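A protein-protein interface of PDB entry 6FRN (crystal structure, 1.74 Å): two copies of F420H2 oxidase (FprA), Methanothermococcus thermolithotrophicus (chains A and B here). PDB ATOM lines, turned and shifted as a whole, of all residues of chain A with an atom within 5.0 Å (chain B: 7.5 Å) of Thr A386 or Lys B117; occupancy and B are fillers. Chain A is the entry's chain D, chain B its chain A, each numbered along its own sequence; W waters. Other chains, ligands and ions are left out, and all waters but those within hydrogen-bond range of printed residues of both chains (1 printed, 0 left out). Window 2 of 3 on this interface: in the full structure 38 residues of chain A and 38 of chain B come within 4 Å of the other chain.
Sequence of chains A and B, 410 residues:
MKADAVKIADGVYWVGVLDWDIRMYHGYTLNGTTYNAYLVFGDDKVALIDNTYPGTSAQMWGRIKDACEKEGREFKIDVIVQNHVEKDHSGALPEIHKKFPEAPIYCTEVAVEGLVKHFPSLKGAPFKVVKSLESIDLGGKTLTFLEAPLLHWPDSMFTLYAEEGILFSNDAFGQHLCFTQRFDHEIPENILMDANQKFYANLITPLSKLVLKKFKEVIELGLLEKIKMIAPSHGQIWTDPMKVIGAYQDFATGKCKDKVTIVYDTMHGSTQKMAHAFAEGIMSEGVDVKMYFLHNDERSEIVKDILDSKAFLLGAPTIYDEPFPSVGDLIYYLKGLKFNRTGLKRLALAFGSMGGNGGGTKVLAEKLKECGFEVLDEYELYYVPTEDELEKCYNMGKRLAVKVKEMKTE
The side-chain amino group of Lys B117 is in salt-bridge range of the side-chain carboxylate of Glu A389, at 2.8 Å. The backbone carbonyl oxygen (O) of Tyr A382 is in hydrogen-bond range of the side-chain amino group (NZ) of Lys B117 (2.7 Å). NZ of Lys B117 lies within hydrogen-bond range of O of Val A384, at 2.8 Å.
ND1 of His B118 sits at hydrogen-bond distance from O of Gly B114, at 2.8 Å. OG1 of Thr A386 sits close to N of Asp A388 (3.4 Å). The backbone NH of Thr A386 lies within hydrogen-bond range of the side-chain carboxylate of Glu A389, at 3.0 Å.
Among the printed residues, pairs that only touch across the chains: Tyr A382 with Gly B114, Tyr A383 with His B118, Thr A386 with Lys B117, Val A384 with His B118, Tyr A383 with Gly B114 and Tyr A382 with Glu B113.
Printed residues of chain B within 4 Å of Tyr A382: Glu B113, Gly B114 and Lys B117. Of the printed residues of chain B, Val A384 touches Lys B117 (2.8 Å) and His B118 (3.9 Å). Thr A386 touches one residue of chain B. Leu A390 touches none of the printed residues of chain B. Of the printed residues of chain A, Glu B113 touches Tyr A382 (3.96 Å). Of the printed residues of chain A, Gly B114 touches Tyr A382 and Tyr A383. Lys B117 touches four residues of chain A. The nearest residue of chain B that does not touch Thr A386 is Pro B120 (6.9 Å). The nearest printed residue of chain B that does not touch Tyr A383 is Lys B117 (4.3 Å).
Of the 10 printed residues of chain A, 5 touch a printed residue of chain B. Among the printed residues, Asp or Glu carboxylates within 4 Å of a Lys or Arg side-chain nitrogen of the other chain: Glu A389 with Lys B117 (2.8 Å).
No position is printed for both chains.
Water W1 lies within hydrogen-bond range of the backbone carbonyl oxygen of Lys B117 (2.6 Å) and the backbone carbonyl oxygen of Val A384 (3.1 Å).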
ATOM      1  N   LEU A 381       0.188  21.259  24.177  1.00  0.00           N
ATOM      2  CA  LEU A 381      -0.301  19.908  23.905  1.00  0.00           C
ATOM      3  C   LEU A 381       0.861  18.958  23.619  1.00  0.00           C
ATOM      4  O   LEU A 381       1.993  19.403  23.426  1.00  0.00           O
ATOM      5  CB  LEU A 381      -1.371  19.880  22.819  1.00  0.00           C
ATOM      6  CG  LEU A 381      -1.044  20.511  21.477  1.00  0.00           C
ATOM      7  CD1 LEU A 381      -0.108  19.641  20.663  1.00  0.00           C
ATOM      8  CD2 LEU A 381      -2.317  20.755  20.679  1.00  0.00           C
ATOM      9  N   TYR A 382       0.559  17.669  23.560  1.00  0.00           N
ATOM     10  CA  TYR A 382       1.532  16.594  23.368  1.00  0.00           C
ATOM     11  C   TYR A 382       1.707  16.228  21.888  1.00  0.00           C
ATOM     12  O   TYR A 382       0.744  15.815  21.256  1.00  0.00           O
ATOM     13  CB  TYR A 382       1.040  15.381  24.150  1.00  0.00           C
ATOM     14  CG  TYR A 382       1.899  14.149  24.059  1.00  0.00           C
ATOM     15  CD1 TYR A 382       3.261  14.208  24.314  1.00  0.00           C
ATOM     16  CD2 TYR A 382       1.328  12.895  23.868  1.00  0.00           C
ATOM     17  CE1 TYR A 382       4.040  13.057  24.343  1.00  0.00           C
ATOM     18  CE2 TYR A 382       2.098  11.738  23.896  1.00  0.00           C
ATOM     19  CZ  TYR A 382       3.451  11.821  24.154  1.00  0.00           C
ATOM     20  OH  TYR A 382       4.223  10.687  24.165  1.00  0.00           O
ATOM     21  N   TYR A 383       2.916  16.382  21.343  1.00  0.00           N
ATOM     22  CA  TYR A 383       3.224  16.034  19.955  1.00  0.00           C
ATOM     23  C   TYR A 383       2.213  16.591  18.922  1.00  0.00           C
ATOM     24  O   TYR A 383       1.922  17.783  18.963  1.00  0.00           O
ATOM     25  CB  TYR A 383       3.423  14.503  19.795  1.00  0.00           C
ATOM     26  CG  TYR A 383       4.641  13.947  20.497  1.00  0.00           C
ATOM     27  CD1 TYR A 383       5.885  14.541  20.345  1.00  0.00           C
ATOM     28  CD2 TYR A 383       4.585  12.733  21.161  1.00  0.00           C
ATOM     29  CE1 TYR A 383       7.031  13.974  20.888  1.00  0.00           C
ATOM     30  CE2 TYR A 383       5.727  12.151  21.705  1.00  0.00           C
ATOM     31  CZ  TYR A 383       6.941  12.800  21.607  1.00  0.00           C
ATOM     32  OH  TYR A 383       8.083  12.274  22.162  1.00  0.00           O
ATOM     33  N   VAL A 384       1.684  15.756  18.002  1.00  0.00           N
ATOM     34  CA  VAL A 384       0.851  16.230  16.907  1.00  0.00           C
ATOM     35  C   VAL A 384      -0.552  16.487  17.408  1.00  0.00           C
ATOM     36  O   VAL A 384      -1.149  15.576  17.976  1.00  0.00           O
ATOM     37  CB  VAL A 384       0.858  15.204  15.736  1.00  0.00           C
ATOM     38  CG1 VAL A 384       0.038  15.704  14.550  1.00  0.00           C
ATOM     39  CG2 VAL A 384       2.289  14.887  15.297  1.00  0.00           C
ATOM     40  N   PRO A 385      -1.136  17.672  17.133  1.00  0.00           N
ATOM     41  CA  PRO A 385      -2.509  17.902  17.586  1.00  0.00           C
ATOM     42  C   PRO A 385      -3.511  16.960  16.926  1.00  0.00           C
ATOM     43  O   PRO A 385      -3.416  16.693  15.728  1.00  0.00           O
ATOM     44  CB  PRO A 385      -2.803  19.345  17.151  1.00  0.00           C
ATOM     45  CG  PRO A 385      -1.525  19.949  16.807  1.00  0.00           C
ATOM     46  CD  PRO A 385      -0.579  18.860  16.462  1.00  0.00           C
ATOM     47  N   THR A 386      -4.490  16.510  17.684  1.00  0.00           N
ATOM     48  CA  THR A 386      -5.582  15.736  17.136  1.00  0.00           C
ATOM     49  C   THR A 386      -6.563  16.751  16.534  1.00  0.00           C
ATOM     50  O   THR A 386      -6.433  17.958  16.781  1.00  0.00           O
ATOM     51  CB  THR A 386      -6.325  14.968  18.236  1.00  0.00           C
ATOM     52  OG1 THR A 386      -6.918  15.930  19.096  1.00  0.00           O
ATOM     53  CG2 THR A 386      -5.403  14.059  19.051  1.00  0.00           C
ATOM     54  N   GLU A 387      -7.590  16.262  15.845  1.00  0.00           N
ATOM     55  CA  GLU A 387      -8.633  17.122  15.277  1.00  0.00           C
ATOM     56  C   GLU A 387      -9.324  17.926  16.382  1.00  0.00           C
ATOM     57  O   GLU A 387      -9.549  19.118  16.212  1.00  0.00           O
ATOM     58  CB  GLU A 387      -9.676  16.255  14.529  1.00  0.00           C
ATOM     59  CG  GLU A 387     -10.600  17.032  13.612  1.00  0.00           C
ATOM     60  CD  GLU A 387     -10.124  17.107  12.173  1.00  0.00           C
ATOM     61  OE1 GLU A 387      -8.900  17.261  11.956  1.00  0.00           O
ATOM     62  OE2 GLU A 387     -10.979  17.016  11.260  1.00  0.00           O
ATOM     63  N   ASP A 388      -9.641  17.283  17.520  1.00  0.00           N
ATOM     64  CA  ASP A 388     -10.260  17.973  18.644  1.00  0.00           C
ATOM     65  C   ASP A 388      -9.337  19.053  19.227  1.00  0.00           C
ATOM     66  O   ASP A 388      -9.825  20.100  19.628  1.00  0.00           O
ATOM     67  CB  ASP A 388     -10.659  16.998  19.757  1.00  0.00           C
ATOM     68  CG  ASP A 388     -11.803  16.081  19.382  1.00  0.00           C
ATOM     69  OD1 ASP A 388     -12.485  16.367  18.379  1.00  0.00           O
ATOM     70  OD2 ASP A 388     -12.011  15.080  20.084  1.00  0.00           O
ATOM     71  N   GLU A 389      -8.027  18.802  19.311  1.00  0.00           N
ATOM     72  CA  GLU A 389      -7.116  19.827  19.832  1.00  0.00           C
ATOM     73  C   GLU A 389      -7.026  21.033  18.892  1.00  0.00           C
ATOM     74  O   GLU A 389      -6.897  22.162  19.361  1.00  0.00           O
ATOM     75  CB  GLU A 389      -5.744  19.241  20.113  1.00  0.00           C
ATOM     76  CG  GLU A 389      -5.802  18.279  21.282  1.00  0.00           C
ATOM     77  CD  GLU A 389      -4.549  17.472  21.541  1.00  0.00           C
ATOM     78  OE1 GLU A 389      -3.852  17.083  20.575  1.00  0.00           O
ATOM     79  OE2 GLU A 389      -4.295  17.176  22.727  1.00  0.00           O
ATOM     80  N   LEU A 390      -7.108  20.802  17.565  1.00  0.00           N
ATOM     81  CA  LEU A 390      -7.119  21.898  16.607  1.00  0.00           C
ATOM     82  C   LEU A 390      -8.425  22.665  16.726  1.00  0.00           C
ATOM     83  O   LEU A 390      -8.414  23.891  16.529  1.00  0.00           O
ATOM     84  CB  LEU A 390      -6.900  21.409  15.168  1.00  0.00           C
ATOM     85  CG  LEU A 390      -5.518  20.790  14.894  1.00  0.00           C
ATOM     86  CD1 LEU A 390      -5.424  20.276  13.477  1.00  0.00           C
ATOM     87  CD2 LEU A 390      -4.413  21.777  15.152  1.00  0.00           C
ATOM     88  N   ALA B 111       6.303   5.093  24.343  1.00  0.00           N
ATOM     89  CA  ALA B 111       6.426   5.192  22.904  1.00  0.00           C
ATOM     90  C   ALA B 111       5.157   4.787  22.174  1.00  0.00           C
ATOM     91  O   ALA B 111       4.831   5.387  21.160  1.00  0.00           O
ATOM     92  CB  ALA B 111       7.619   4.394  22.396  1.00  0.00           C
ATOM     93  N   VAL B 112       4.415   3.801  22.704  1.00  0.00           N
ATOM     94  CA  VAL B 112       3.168   3.390  22.074  1.00  0.00           C
ATOM     95  C   VAL B 112       2.264   4.619  21.984  1.00  0.00           C
ATOM     96  O   VAL B 112       1.657   4.853  20.944  1.00  0.00           O
ATOM     97  CB  VAL B 112       2.432   2.251  22.836  1.00  0.00           C
ATOM     98  CG1 VAL B 112       1.050   2.008  22.243  1.00  0.00           C
ATOM     99  CG2 VAL B 112       3.252   0.957  22.844  1.00  0.00           C
ATOM    100  N   GLU B 113       2.163   5.388  23.090  1.00  0.00           N
ATOM    101  CA  GLU B 113       1.297   6.571  23.135  1.00  0.00           C
ATOM    102  C   GLU B 113       1.766   7.642  22.152  1.00  0.00           C
ATOM    103  O   GLU B 113       0.951   8.224  21.427  1.00  0.00           O
ATOM    104  CB  GLU B 113       1.251   7.132  24.564  1.00  0.00           C
ATOM    105  CG  GLU B 113       0.037   7.988  24.831  1.00  0.00           C
ATOM    106  CD  GLU B 113       0.091   8.709  26.160  1.00  0.00           C
ATOM    107  OE1 GLU B 113      -0.458   9.832  26.242  1.00  0.00           O
ATOM    108  OE2 GLU B 113       0.682   8.153  27.115  1.00  0.00           O
ATOM    109  N   GLY B 114       3.065   7.918  22.163  1.00  0.00           N
ATOM    110  CA  GLY B 114       3.643   8.926  21.290  1.00  0.00           C
ATOM    111  C   GLY B 114       3.522   8.573  19.815  1.00  0.00           C
ATOM    112  O   GLY B 114       3.212   9.440  18.994  1.00  0.00           O
ATOM    113  N   LEU B 115       3.717   7.299  19.461  1.00  0.00           N
ATOM    114  CA  LEU B 115       3.598   6.859  18.054  1.00  0.00           C
ATOM    115  C   LEU B 115       2.185   6.973  17.537  1.00  0.00           C
ATOM    116  O   LEU B 115       1.999   7.415  16.402  1.00  0.00           O
ATOM    117  CB  LEU B 115       4.104   5.425  17.871  1.00  0.00           C
ATOM    118  CG  LEU B 115       5.606   5.246  18.010  1.00  0.00           C
ATOM    119  CD1 LEU B 115       5.959   3.805  18.248  1.00  0.00           C
ATOM    120  CD2 LEU B 115       6.364   5.841  16.818  1.00  0.00           C
ATOM    121  N   VAL B 116       1.174   6.567  18.341  1.00  0.00           N
ATOM    122  CA  VAL B 116      -0.211   6.647  17.911  1.00  0.00           C
ATOM    123  C   VAL B 116      -0.636   8.112  17.830  1.00  0.00           C
ATOM    124  O   VAL B 116      -1.432   8.446  16.964  1.00  0.00           O
ATOM    125  CB  VAL B 116      -1.153   5.824  18.819  1.00  0.00           C
ATOM    126  CG1 VAL B 116      -2.615   6.011  18.409  1.00  0.00           C
ATOM    127  CG2 VAL B 116      -0.773   4.350  18.773  1.00  0.00           C
ATOM    128  N   LYS B 117      -0.085   8.985  18.683  1.00  0.00           N
ATOM    129  CA  LYS B 117      -0.427  10.410  18.618  1.00  0.00           C
ATOM    130  C   LYS B 117       0.110  10.999  17.292  1.00  0.00           C
ATOM    131  O   LYS B 117      -0.573  11.779  16.642  1.00  0.00           O
ATOM    132  CB  LYS B 117       0.143  11.184  19.809  1.00  0.00           C
ATOM    133  CG  LYS B 117      -0.471  12.595  19.938  1.00  0.00           C
ATOM    134  CD  LYS B 117      -1.393  12.729  21.084  1.00  0.00           C
ATOM    135  CE  LYS B 117      -2.422  13.806  20.932  1.00  0.00           C
ATOM    136  NZ  LYS B 117      -1.849  15.144  20.697  1.00  0.00           N
ATOM    137  N   HIS B 118       1.315  10.605  16.891  1.00  0.00           N
ATOM    138  CA  HIS B 118       1.879  11.029  15.603  1.00  0.00           C
ATOM    139  C   HIS B 118       1.098  10.407  14.449  1.00  0.00           C
ATOM    140  O   HIS B 118       0.773  11.095  13.481  1.00  0.00           O
ATOM    141  CB  HIS B 118       3.349  10.574  15.468  1.00  0.00           C
ATOM    142  CG  HIS B 118       4.380  11.445  16.125  1.00  0.00           C
ATOM    143  ND1 HIS B 118       4.719  11.301  17.451  1.00  0.00           N
ATOM    144  CD2 HIS B 118       5.200  12.367  15.575  1.00  0.00           C
ATOM    145  CE1 HIS B 118       5.707  12.163  17.679  1.00  0.00           C
ATOM    146  NE2 HIS B 118       6.019  12.833  16.586  1.00  0.00           N
ATOM    147  N   PHE B 119       0.820   9.084  14.542  1.00  0.00           N
ATOM    148  CA  PHE B 119       0.256   8.291  13.458  1.00  0.00           C
ATOM    149  C   PHE B 119      -0.994   7.551  13.895  1.00  0.00           C
ATOM    150  O   PHE B 119      -0.914   6.389  14.283  1.00  0.00           O
ATOM    151  CB  PHE B 119       1.336   7.304  12.971  1.00  0.00           C
ATOM    152  CG  PHE B 119       2.708   7.923  12.791  1.00  0.00           C
ATOM    153  CD1 PHE B 119       2.912   8.936  11.869  1.00  0.00           C
ATOM    154  CD2 PHE B 119       3.790   7.498  13.555  1.00  0.00           C
ATOM    155  CE1 PHE B 119       4.161   9.526  11.731  1.00  0.00           C
ATOM    156  CE2 PHE B 119       5.038   8.099  13.417  1.00  0.00           C
ATOM    157  CZ  PHE B 119       5.212   9.118  12.519  1.00  0.00           C
ATOM    158  N   PRO B 120      -2.182   8.165  13.758  1.00  0.00           N
ATOM    159  CA  PRO B 120      -3.414   7.485  14.200  1.00  0.00           C
ATOM    160  C   PRO B 120      -3.735   6.163  13.516  1.00  0.00           C
ATOM    161  O   PRO B 120      -4.458   5.364  14.098  1.00  0.00           O
ATOM    162  CB  PRO B 120      -4.516   8.525  13.944  1.00  0.00           C
ATOM    163  CG  PRO B 120      -3.817   9.812  13.806  1.00  0.00           C
ATOM    164  CD  PRO B 120      -2.460   9.532  13.290  1.00  0.00           C
ATOM    165  N   LEU B 122      -1.896   3.733  13.327  1.00  0.00           N
ATOM    166  CA  LEU B 122      -1.263   2.696  14.139  1.00  0.00           C
ATOM    167  C   LEU B 122      -2.126   2.276  15.320  1.00  0.00           C
ATOM    168  O   LEU B 122      -1.717   1.378  16.065  1.00  0.00           O
ATOM    169  CB  LEU B 122       0.107   3.135  14.656  1.00  0.00           C
ATOM    170  CG  LEU B 122       1.169   3.416  13.620  1.00  0.00           C
ATOM    171  CD1 LEU B 122       2.452   3.869  14.310  1.00  0.00           C
ATOM    172  CD2 LEU B 122       1.451   2.179  12.758  1.00  0.00           C
HETATM  173  O   HOH W   1      -2.693  13.338  16.563  1.00  0.00           O
